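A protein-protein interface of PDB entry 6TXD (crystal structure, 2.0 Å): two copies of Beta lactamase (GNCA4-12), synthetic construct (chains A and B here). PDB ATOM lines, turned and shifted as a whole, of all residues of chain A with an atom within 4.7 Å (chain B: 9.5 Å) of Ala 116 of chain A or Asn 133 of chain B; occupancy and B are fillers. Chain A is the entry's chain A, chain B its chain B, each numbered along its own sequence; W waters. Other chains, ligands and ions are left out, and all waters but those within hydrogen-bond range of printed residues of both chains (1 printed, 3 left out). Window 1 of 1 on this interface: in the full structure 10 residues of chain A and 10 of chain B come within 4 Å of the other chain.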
ATOM      1  N   ARG A  58     -14.328  20.995 -11.412  1.00  0.00           N
ATOM      2  CA  ARG A  58     -13.794  19.663 -11.675  1.00  0.00           C
ATOM      3  C   ARG A  58     -14.733  18.576 -11.161  1.00  0.00           C
ATOM      4  O   ARG A  58     -14.739  17.462 -11.695  1.00  0.00           O
ATOM      5  CB  ARG A  58     -12.403  19.525 -11.053  1.00  0.00           C
ATOM      6  CG  ARG A  58     -11.342  20.366 -11.754  1.00  0.00           C
ATOM      7  CD  ARG A  58      -9.963  20.180 -11.135  1.00  0.00           C
ATOM      8  NE  ARG A  58      -9.587  18.774 -11.027  1.00  0.00           N
ATOM      9  CZ  ARG A  58      -9.187  18.023 -12.048  1.00  0.00           C
ATOM     10  NH1 ARG A  58      -9.108  18.539 -13.267  1.00  0.00           N
ATOM     11  NH2 ARG A  58      -8.865  16.752 -11.851  1.00  0.00           N
ATOM     12  N   LYS A  63     -14.090  14.766 -12.770  1.00  0.00           N
ATOM     13  CA  LYS A  63     -12.690  14.515 -12.485  1.00  0.00           C
ATOM     14  C   LYS A  63     -12.399  14.638 -10.998  1.00  0.00           C
ATOM     15  O   LYS A  63     -11.263  14.406 -10.574  1.00  0.00           O
ATOM     16  CB  LYS A  63     -11.809  15.494 -13.273  1.00  0.00           C
ATOM     17  CG  LYS A  63     -12.114  15.562 -14.769  1.00  0.00           C
ATOM     18  CD  LYS A  63     -11.331  16.696 -15.425  1.00  0.00           C
ATOM     19  CE  LYS A  63     -11.703  16.855 -16.889  1.00  0.00           C
ATOM     20  NZ  LYS A  63     -11.313  15.666 -17.699  1.00  0.00           N
ATOM     21  N   GLU A  64     -13.402  15.004 -10.200  1.00  0.00           N
ATOM     22  CA  GLU A  64     -13.231  15.200  -8.767  1.00  0.00           C
ATOM     23  C   GLU A  64     -14.508  14.773  -8.052  1.00  0.00           C
ATOM     24  O   GLU A  64     -15.602  14.821  -8.621  1.00  0.00           O
ATOM     25  CB  GLU A  64     -12.878  16.665  -8.448  1.00  0.00           C
ATOM     26  CG  GLU A  64     -12.634  16.987  -6.973  1.00  0.00           C
ATOM     27  CD  GLU A  64     -11.502  16.176  -6.366  1.00  0.00           C
ATOM     28  OE1 GLU A  64     -10.362  16.684  -6.320  1.00  0.00           O
ATOM     29  OE2 GLU A  64     -11.753  15.033  -5.928  1.00  0.00           O
ATOM     30  N   ARG A  68     -14.339  12.518  -1.754  1.00  0.00           N
ATOM     31  CA  ARG A  68     -12.979  11.993  -1.729  1.00  0.00           C
ATOM     32  C   ARG A  68     -12.246  12.479  -0.486  1.00  0.00           C
ATOM     33  O   ARG A  68     -12.265  13.670  -0.163  1.00  0.00           O
ATOM     34  CB  ARG A  68     -12.223  12.417  -2.990  1.00  0.00           C
ATOM     35  CG  ARG A  68     -10.803  11.878  -3.071  1.00  0.00           C
ATOM     36  CD  ARG A  68     -10.163  12.186  -4.418  1.00  0.00           C
ATOM     37  NE  ARG A  68      -9.919  13.614  -4.603  1.00  0.00           N
ATOM     38  CZ  ARG A  68      -8.811  14.240  -4.217  1.00  0.00           C
ATOM     39  NH1 ARG A  68      -7.840  13.566  -3.618  1.00  0.00           N
ATOM     40  NH2 ARG A  68      -8.675  15.543  -4.426  1.00  0.00           N
ATOM     41  N   LEU A 112      -4.259  22.172   0.526  1.00  0.00           N
ATOM     42  CA  LEU A 112      -4.635  20.832   0.090  1.00  0.00           C
ATOM     43  C   LEU A 112      -5.514  20.883  -1.153  1.00  0.00           C
ATOM     44  O   LEU A 112      -5.395  20.030  -2.040  1.00  0.00           O
ATOM     45  CB  LEU A 112      -5.348  20.093   1.221  1.00  0.00           C
ATOM     46  CG  LEU A 112      -4.497  19.700   2.431  1.00  0.00           C
ATOM     47  CD1 LEU A 112      -5.383  19.183   3.555  1.00  0.00           C
ATOM     48  CD2 LEU A 112      -3.455  18.661   2.044  1.00  0.00           C
ATOM     49  N   LEU A 113      -6.404  21.874  -1.233  1.00  0.00           N
ATOM     50  CA  LEU A 113      -7.252  22.011  -2.414  1.00  0.00           C
ATOM     51  C   LEU A 113      -6.447  22.494  -3.614  1.00  0.00           C
ATOM     52  O   LEU A 113      -6.712  22.082  -4.750  1.00  0.00           O
ATOM     53  CB  LEU A 113      -8.408  22.965  -2.121  1.00  0.00           C
ATOM     54  CG  LEU A 113      -9.435  22.482  -1.092  1.00  0.00           C
ATOM     55  CD1 LEU A 113     -10.382  23.608  -0.708  1.00  0.00           C
ATOM     56  CD2 LEU A 113     -10.207  21.281  -1.618  1.00  0.00           C
ATOM     57  N   LEU A 114      -5.468  23.374  -3.385  1.00  0.00           N
ATOM     58  CA  LEU A 114      -4.565  23.769  -4.460  1.00  0.00           C
ATOM     59  C   LEU A 114      -3.801  22.565  -4.994  1.00  0.00           C
ATOM     60  O   LEU A 114      -3.625  22.419  -6.210  1.00  0.00           O
ATOM     61  CB  LEU A 114      -3.594  24.839  -3.961  1.00  0.00           C
ATOM     62  CG  LEU A 114      -4.108  26.278  -3.955  1.00  0.00           C
ATOM     63  CD1 LEU A 114      -3.195  27.166  -3.122  1.00  0.00           C
ATOM     64  CD2 LEU A 114      -4.224  26.801  -5.377  1.00  0.00           C
ATOM     65  N   GLU A 115      -3.339  21.696  -4.093  1.00  0.00           N
ATOM     66  CA  GLU A 115      -2.730  20.436  -4.504  1.00  0.00           C
ATOM     67  C   GLU A 115      -3.689  19.619  -5.359  1.00  0.00           C
ATOM     68  O   GLU A 115      -3.287  19.039  -6.376  1.00  0.00           O
ATOM     69  CB  GLU A 115      -2.313  19.645  -3.265  1.00  0.00           C
ATOM     70  CG  GLU A 115      -0.979  18.938  -3.367  1.00  0.00           C
ATOM     71  CD  GLU A 115      -0.399  18.626  -2.003  1.00  0.00           C
ATOM     72  OE1 GLU A 115       0.796  18.275  -1.928  1.00  0.00           O
ATOM     73  OE2 GLU A 115      -1.140  18.740  -1.002  1.00  0.00           O
ATOM     74  N   ALA A 116      -4.965  19.568  -4.967  1.00  0.00           N
ATOM     75  CA  ALA A 116      -5.954  18.821  -5.734  1.00  0.00           C
ATOM     76  C   ALA A 116      -6.171  19.428  -7.115  1.00  0.00           C
ATOM     77  O   ALA A 116      -6.507  18.705  -8.061  1.00  0.00           O
ATOM     78  CB  ALA A 116      -7.275  18.759  -4.968  1.00  0.00           C
ATOM     79  N   LEU A 117      -5.993  20.743  -7.249  1.00  0.00           N
ATOM     80  CA  LEU A 117      -6.084  21.387  -8.554  1.00  0.00           C
ATOM     81  C   LEU A 117      -4.849  21.136  -9.405  1.00  0.00           C
ATOM     82  O   LEU A 117      -4.948  21.077 -10.635  1.00  0.00           O
ATOM     83  CB  LEU A 117      -6.268  22.897  -8.395  1.00  0.00           C
ATOM     84  CG  LEU A 117      -7.622  23.473  -7.994  1.00  0.00           C
ATOM     85  CD1 LEU A 117      -7.630  24.963  -8.287  1.00  0.00           C
ATOM     86  CD2 LEU A 117      -8.753  22.771  -8.723  1.00  0.00           C
ATOM     87  N   GLY A 118      -3.690  21.000  -8.776  1.00  0.00           N
ATOM     88  CA  GLY A 118      -2.433  20.989  -9.485  1.00  0.00           C
ATOM     89  C   GLY A 118      -1.608  22.249  -9.339  1.00  0.00           C
ATOM     90  O   GLY A 118      -0.686  22.456 -10.135  1.00  0.00           O
ATOM     91  N   ARG B  40       1.665  10.166   1.186  1.00  0.00           N
ATOM     92  CA  ARG B  40       2.495  10.591   0.069  1.00  0.00           C
ATOM     93  C   ARG B  40       3.902  10.022   0.188  1.00  0.00           C
ATOM     94  O   ARG B  40       4.485   9.980   1.276  1.00  0.00           O
ATOM     95  CB  ARG B  40       2.549  12.118  -0.008  1.00  0.00           C
ATOM     96  CG  ARG B  40       1.283  12.742  -0.573  1.00  0.00           C
ATOM     97  CD  ARG B  40       1.433  14.242  -0.784  1.00  0.00           C
ATOM     98  NE  ARG B  40       0.232  14.821  -1.381  1.00  0.00           N
ATOM     99  CZ  ARG B  40      -0.001  14.874  -2.689  1.00  0.00           C
ATOM    100  NH1 ARG B  40       0.887  14.386  -3.545  1.00  0.00           N
ATOM    101  NH2 ARG B  40      -1.123  15.415  -3.142  1.00  0.00           N
ATOM    102  N   THR B 124       1.640  17.195 -14.606  1.00  0.00           N
ATOM    103  CA  THR B 124       0.623  17.273 -13.562  1.00  0.00           C
ATOM    104  C   THR B 124      -0.742  17.611 -14.151  1.00  0.00           C
ATOM    105  O   THR B 124      -1.767  17.073 -13.712  1.00  0.00           O
ATOM    106  CB  THR B 124       1.029  18.309 -12.513  1.00  0.00           C
ATOM    107  OG1 THR B 124       2.322  17.980 -11.990  1.00  0.00           O
ATOM    108  CG2 THR B 124       0.021  18.345 -11.373  1.00  0.00           C
ATOM    109  N   ALA B 125      -0.773  18.490 -15.156  1.00  0.00           N
ATOM    110  CA  ALA B 125      -2.036  18.837 -15.799  1.00  0.00           C
ATOM    111  C   ALA B 125      -2.646  17.632 -16.504  1.00  0.00           C
ATOM    112  O   ALA B 125      -3.869  17.444 -16.480  1.00  0.00           O
ATOM    113  CB  ALA B 125      -1.828  19.987 -16.783  1.00  0.00           C
ATOM    114  N   PHE B 126      -1.812  16.805 -17.142  1.00  0.00           N
ATOM    115  CA  PHE B 126      -2.319  15.591 -17.774  1.00  0.00           C
ATOM    116  C   PHE B 126      -2.932  14.650 -16.745  1.00  0.00           C
ATOM    117  O   PHE B 126      -3.980  14.043 -16.992  1.00  0.00           O
ATOM    118  CB  PHE B 126      -1.201  14.884 -18.539  1.00  0.00           C
ATOM    119  CG  PHE B 126      -1.542  13.478 -18.949  1.00  0.00           C
ATOM    120  CD1 PHE B 126      -2.389  13.241 -20.020  1.00  0.00           C
ATOM    121  CD2 PHE B 126      -1.021  12.393 -18.261  1.00  0.00           C
ATOM    122  CE1 PHE B 126      -2.708  11.948 -20.398  1.00  0.00           C
ATOM    123  CE2 PHE B 126      -1.336  11.101 -18.634  1.00  0.00           C
ATOM    124  CZ  PHE B 126      -2.181  10.878 -19.704  1.00  0.00           C
ATOM    125  N   LEU B 127      -2.290  14.519 -15.582  1.00  0.00           N
ATOM    126  CA  LEU B 127      -2.808  13.627 -14.550  1.00  0.00           C
ATOM    127  C   LEU B 127      -4.120  14.147 -13.976  1.00  0.00           C
ATOM    128  O   LEU B 127      -5.023  13.361 -13.669  1.00  0.00           O
ATOM    129  CB  LEU B 127      -1.763  13.444 -13.450  1.00  0.00           C
ATOM    130  CG  LEU B 127      -0.510  12.692 -13.906  1.00  0.00           C
ATOM    131  CD1 LEU B 127       0.626  12.859 -12.910  1.00  0.00           C
ATOM    132  CD2 LEU B 127      -0.823  11.220 -14.130  1.00  0.00           C
ATOM    133  N   ARG B 128      -4.247  15.468 -13.823  1.00  0.00           N
ATOM    134  CA  ARG B 128      -5.524  16.034 -13.402  1.00  0.00           C
ATOM    135  C   ARG B 128      -6.607  15.796 -14.447  1.00  0.00           C
ATOM    136  O   ARG B 128      -7.775  15.592 -14.096  1.00  0.00           O
ATOM    137  CB  ARG B 128      -5.378  17.532 -13.128  1.00  0.00           C
ATOM    138  CG  ARG B 128      -4.500  17.875 -11.933  1.00  0.00           C
ATOM    139  CD  ARG B 128      -5.039  17.270 -10.644  1.00  0.00           C
ATOM    140  NE  ARG B 128      -4.130  17.485  -9.521  1.00  0.00           N
ATOM    141  CZ  ARG B 128      -3.058  16.738  -9.275  1.00  0.00           C
ATOM    142  NH1 ARG B 128      -2.760  15.720 -10.071  1.00  0.00           N
ATOM    143  NH2 ARG B 128      -2.283  17.006  -8.233  1.00  0.00           N
ATOM    144  N   SER B 129      -6.237  15.805 -15.730  1.00  0.00           N
ATOM    145  CA  SER B 129      -7.214  15.624 -16.797  1.00  0.00           C
ATOM    146  C   SER B 129      -7.799  14.218 -16.825  1.00  0.00           C
ATOM    147  O   SER B 129      -8.880  14.024 -17.391  1.00  0.00           O
ATOM    148  CB  SER B 129      -6.579  15.950 -18.151  1.00  0.00           C
ATOM    149  OG  SER B 129      -5.701  14.917 -18.564  1.00  0.00           O
ATOM    150  N   ILE B 130      -7.120  13.235 -16.233  1.00  0.00           N
ATOM    151  CA  ILE B 130      -7.615  11.863 -16.212  1.00  0.00           C
ATOM    152  C   ILE B 130      -8.167  11.476 -14.843  1.00  0.00           C
ATOM    153  O   ILE B 130      -8.479  10.303 -14.616  1.00  0.00           O
ATOM    154  CB  ILE B 130      -6.531  10.872 -16.665  1.00  0.00           C
ATOM    155  CG1 ILE B 130      -5.336  10.901 -15.711  1.00  0.00           C
ATOM    156  CG2 ILE B 130      -6.086  11.188 -18.085  1.00  0.00           C
ATOM    157  CD1 ILE B 130      -4.365   9.757 -15.918  1.00  0.00           C
ATOM    158  N   GLY B 131      -8.298  12.430 -13.928  1.00  0.00           N
ATOM    159  CA  GLY B 131      -8.897  12.160 -12.639  1.00  0.00           C
ATOM    160  C   GLY B 131      -7.934  11.835 -11.521  1.00  0.00           C
ATOM    161  O   GLY B 131      -8.384  11.455 -10.433  1.00  0.00           O
ATOM    162  N   ASP B 132      -6.629  11.957 -11.750  1.00  0.00           N
ATOM    163  CA  ASP B 132      -5.636  11.801 -10.687  1.00  0.00           C
ATOM    164  C   ASP B 132      -5.443  13.168 -10.047  1.00  0.00           C
ATOM    165  O   ASP B 132      -4.726  14.020 -10.575  1.00  0.00           O
ATOM    166  CB  ASP B 132      -4.328  11.240 -11.235  1.00  0.00           C
ATOM    167  CG  ASP B 132      -3.330  10.885 -10.138  1.00  0.00           C
ATOM    168  OD1 ASP B 132      -3.422  11.440  -9.021  1.00  0.00           O
ATOM    169  OD2 ASP B 132      -2.442  10.045 -10.395  1.00  0.00           O
ATOM    170  N   ASN B 133      -6.087  13.377  -8.899  1.00  0.00           N
ATOM    171  CA  ASN B 133      -6.019  14.637  -8.173  1.00  0.00           C
ATOM    172  C   ASN B 133      -4.985  14.604  -7.054  1.00  0.00           C
ATOM    173  O   ASN B 133      -5.023  15.453  -6.157  1.00  0.00           O
ATOM    174  CB  ASN B 133      -7.395  14.990  -7.611  1.00  0.00           C
ATOM    175  CG  ASN B 133      -8.486  14.933  -8.662  1.00  0.00           C
ATOM    176  OD1 ASN B 133      -8.338  15.475  -9.757  1.00  0.00           O
ATOM    177  ND2 ASN B 133      -9.588  14.267  -8.336  1.00  0.00           N
ATOM    178  N   VAL B 134      -4.058  13.647  -7.092  1.00  0.00           N
ATOM    179  CA  VAL B 134      -3.114  13.408  -6.009  1.00  0.00           C
ATOM    180  C   VAL B 134      -1.670  13.518  -6.488  1.00  0.00           C
ATOM    181  O   VAL B 134      -0.855  14.221  -5.884  1.00  0.00           O
ATOM    182  CB  VAL B 134      -3.362  12.035  -5.343  1.00  0.00           C
ATOM    183  CG1 VAL B 134      -2.237  11.699  -4.385  1.00  0.00           C
ATOM    184  CG2 VAL B 134      -4.705  12.027  -4.628  1.00  0.00           C
ATOM    185  N   THR B 135      -1.336  12.822  -7.572  1.00  0.00           N
ATOM    186  CA  THR B 135       0.036  12.803  -8.059  1.00  0.00           C
ATOM    187  C   THR B 135       0.440  14.173  -8.592  1.00  0.00           C
ATOM    188  O   THR B 135      -0.330  14.841  -9.287  1.00  0.00           O
ATOM    189  CB  THR B 135       0.194  11.747  -9.155  1.00  0.00           C
ATOM    190  OG1 THR B 135      -0.238  10.474  -8.661  1.00  0.00           O
ATOM    191  CG2 THR B 135       1.647  11.641  -9.596  1.00  0.00           C
ATOM    192  N   ARG B 136       1.659  14.592  -8.257  1.00  0.00           N
ATOM    193  CA  ARG B 136       2.196  15.864  -8.711  1.00  0.00           C
ATOM    194  C   ARG B 136       3.672  15.708  -9.042  1.00  0.00           C
ATOM    195  O   ARG B 136       4.410  15.030  -8.322  1.00  0.00           O
ATOM    196  CB  ARG B 136       2.015  16.964  -7.652  1.00  0.00           C
ATOM    197  CG  ARG B 136       2.632  16.630  -6.299  1.00  0.00           C
ATOM    198  CD  ARG B 136       2.325  17.698  -5.261  1.00  0.00           C
ATOM    199  NE  ARG B 136       3.157  18.887  -5.430  1.00  0.00           N
ATOM    200  CZ  ARG B 136       3.150  19.924  -4.599  1.00  0.00           C
ATOM    201  NH1 ARG B 136       2.356  19.918  -3.537  1.00  0.00           N
ATOM    202  NH2 ARG B 136       3.939  20.966  -4.827  1.00  0.00           N
ATOM    203  N   THR B 155       5.580  13.828  -5.554  1.00  0.00           N
ATOM    204  CA  THR B 155       5.078  12.715  -4.764  1.00  0.00           C
ATOM    205  C   THR B 155       3.808  12.138  -5.374  1.00  0.00           C
ATOM    206  O   THR B 155       3.140  12.763  -6.203  1.00  0.00           O
ATOM    207  CB  THR B 155       4.785  13.134  -3.316  1.00  0.00           C
ATOM    208  OG1 THR B 155       3.804  14.179  -3.307  1.00  0.00           O
ATOM    209  CG2 THR B 155       6.051  13.614  -2.627  1.00  0.00           C
ATOM    210  N   THR B 156       3.491  10.920  -4.938  1.00  0.00           N
ATOM    211  CA  THR B 156       2.218  10.269  -5.204  1.00  0.00           C
ATOM    212  C   THR B 156       1.831   9.492  -3.953  1.00  0.00           C
ATOM    213  O   THR B 156       2.568   9.464  -2.963  1.00  0.00           O
ATOM    214  CB  THR B 156       2.301   9.344  -6.427  1.00  0.00           C
ATOM    215  OG1 THR B 156       0.981   9.033  -6.888  1.00  0.00           O
ATOM    216  CG2 THR B 156       3.025   8.048  -6.074  1.00  0.00           C
ATOM    217  N   THR B 157       0.659   8.873  -3.987  1.00  0.00           N
ATOM    218  CA  THR B 157       0.353   7.872  -2.982  1.00  0.00           C
ATOM    219  C   THR B 157       0.288   6.501  -3.642  1.00  0.00           C
ATOM    220  O   THR B 157       0.032   6.406  -4.847  1.00  0.00           O
ATOM    221  CB  THR B 157      -0.974   8.149  -2.264  1.00  0.00           C
ATOM    222  OG1 THR B 157      -2.068   7.895  -3.154  1.00  0.00           O
ATOM    223  CG2 THR B 157      -1.033   9.589  -1.775  1.00  0.00           C
ATOM    224  N   ALA B 160      -3.138   6.073  -5.328  1.00  0.00           N
ATOM    225  CA  ALA B 160      -3.326   6.905  -6.513  1.00  0.00           C
ATOM    226  C   ALA B 160      -2.527   6.373  -7.696  1.00  0.00           C
ATOM    227  O   ALA B 160      -3.025   6.352  -8.828  1.00  0.00           O
ATOM    228  CB  ALA B 160      -2.938   8.352  -6.210  1.00  0.00           C
ATOM    229  N   MET B 161      -1.288   5.938  -7.455  1.00  0.00           N
ATOM    230  CA  MET B 161      -0.460   5.430  -8.545  1.00  0.00           C
ATOM    231  C   MET B 161      -1.030   4.138  -9.118  1.00  0.00           C
ATOM    232  O   MET B 161      -1.042   3.948 -10.341  1.00  0.00           O
ATOM    233  CB  MET B 161       0.973   5.215  -8.062  1.00  0.00           C
ATOM    234  CG  MET B 161       1.909   4.683  -9.135  1.00  0.00           C
ATOM    235  SD  MET B 161       2.087   5.816 -10.528  1.00  0.00           S
ATOM    236  CE  MET B 161       3.196   7.036  -9.830  1.00  0.00           C
ATOM    237  N   ALA B 163      -4.209   3.189  -9.063  1.00  0.00           N
ATOM    238  CA  ALA B 163      -5.430   3.522  -9.787  1.00  0.00           C
ATOM    239  C   ALA B 163      -5.122   4.234 -11.100  1.00  0.00           C
ATOM    240  O   ALA B 163      -5.804   4.010 -12.107  1.00  0.00           O
ATOM    241  CB  ALA B 163      -6.343   4.377  -8.909  1.00  0.00           C
ATOM    242  N   THR B 164      -4.099   5.092 -11.112  1.00  0.00           N
ATOM    243  CA  THR B 164      -3.736   5.784 -12.345  1.00  0.00           C
ATOM    244  C   THR B 164      -3.130   4.822 -13.360  1.00  0.00           C
ATOM    245  O   THR B 164      -3.480   4.862 -14.546  1.00  0.00           O
ATOM    246  CB  THR B 164      -2.768   6.930 -12.045  1.00  0.00           C
ATOM    247  OG1 THR B 164      -3.449   7.946 -11.298  1.00  0.00           O
ATOM    248  CG2 THR B 164      -2.235   7.534 -13.337  1.00  0.00           C
HETATM  249  O   HOH W   1      -5.835  15.782  -3.598  1.00  0.00           O
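The side-chain amino group of Lys 63 of chain A lies within hydrogen-bond range of the backbone carbonyl oxygen of Ser 129 of chain B, 3.0 Å away.
The guanidinium group (NH2) of Arg 58 of chain A sits at hydrogen-bond distance from the side-chain amide oxygen (OD1) of Asn 133 of chain B (2.5 Å).
NH2 of Arg 58 of chain A lies within hydrogen-bond range of O of Arg 128 of chain B, 2.8 Å away.
OE1 of Glu 115 of chain A lies within salt-bridge range of NE of Arg 40 of chain B (3.5 Å).
NH2 of Arg 128 of chain B sits at hydrogen-bond distance from O of Glu 115 of chain A (2.9 Å).
The backbone carbonyl oxygen (O) of Lys 63 of chain A is in hydrogen-bond range of the side-chain amide nitrogen (ND2) of Asn 133 of chain B.
OE1 of Glu 115 of chain A lies within salt-bridge range of NH1 of Arg 136 of chain B (2.8 Å).
The side-chain carboxylate (OE1) of Glu 64 of chain A lies within hydrogen-bond range of the side-chain amide nitrogen (ND2) of Asn 133 of chain B (3.2 Å).
The backbone carbonyl oxygen of Ala 116 of chain A lies within hydrogen-bond range of the guanidinium group of Arg 128 of chain B, 3.0 Å away.
The backbone carbonyl oxygen (O) of Val 134 of chain B sits at hydrogen-bond distance from the guanidinium group (NH1) of Arg 40 of chain B, 2.9 Å away.
The backbone NH (N) of Arg 136 of chain B sits at hydrogen-bond distance from the backbone carbonyl oxygen (O) of Thr 155 of chain B (3.1 Å).
The backbone carbonyl oxygen of Phe 126 of chain B is in hydrogen-bond range of the side-chain hydroxyl of Ser 129 of chain B (2.5 Å).
O of Arg 58 of chain A lies within hydrogen-bond range of N of Lys 63 of chain A, at 3.0 Å.
OD1 of Asp 132 of chain B lies within hydrogen-bond range of N of Val 134 of chain B, 3.0 Å away.
The side-chain carboxylate of Glu 64 of chain A lies within salt-bridge range of the guanidinium group of Arg 68 of chain A, 2.7 Å away.
Among the printed residues, merely in contact across the chains: Lys 63 of chain A with Arg 128 of chain B, Lys 63 of chain A with Gly 131 of chain B, Arg 68 of chain A with Asn 133 of chain B, Arg 68 of chain A with Val 134 of chain B, Glu 115 of chain A with Asn 133 of chain B, Ala 116 of chain A with Asn 133 of chain B, Leu 117 of chain A with Arg 128 of chain B and Gly 118 of chain A with Arg 128 of chain B.
Of chain B, only Arg 128 and Asn 133 come within 4 Å of Ala 116 of chain A.
Of the printed residues of chain A, Asn 133 of chain B touches Arg 58 (2.5 Å), Lys 63 (2.8 Å), Glu 64 (3.2 Å), Arg 68 (3.5 Å), Glu 115 (3.99 Å) and Ala 116 (3.5 Å).
Of the printed residues of chain B, Gly 118 of chain A touches Arg 128.
Of the printed residues of chain B, Glu 64 of chain A touches Asn 133.
Leu 114 of chain A touches none of the printed residues of chain B.
The nearest printed residue of chain A that does not touch Asn 133 of chain B is Leu 117 of chain A (5.5 Å).
Hydrophobic or aromatic side chains of chain B within 4 Å of the printed part of chain A: Val 134.
Of the 11 printed residues of chain A, 8 touch a printed residue of chain B.
Printed residues of chain A that touch a printed residue of chain B: Arg 58, Lys 63, Glu 64, Arg 68, Glu 115, Ala 116, Leu 117 and Gly 118.
Among the printed residues, 17 pairs touch across the chains.
No position is printed for both chains.
Of the 17 pairs that touch across the chains among the printed residues, none has its exchanged pair printed and touching as well.
Water W1 lies within hydrogen-bond range of the backbone carbonyl oxygen of Asn 133 of chain B (2.7 Å) and the guanidinium group of Arg 68 of chain A (3.0 Å).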
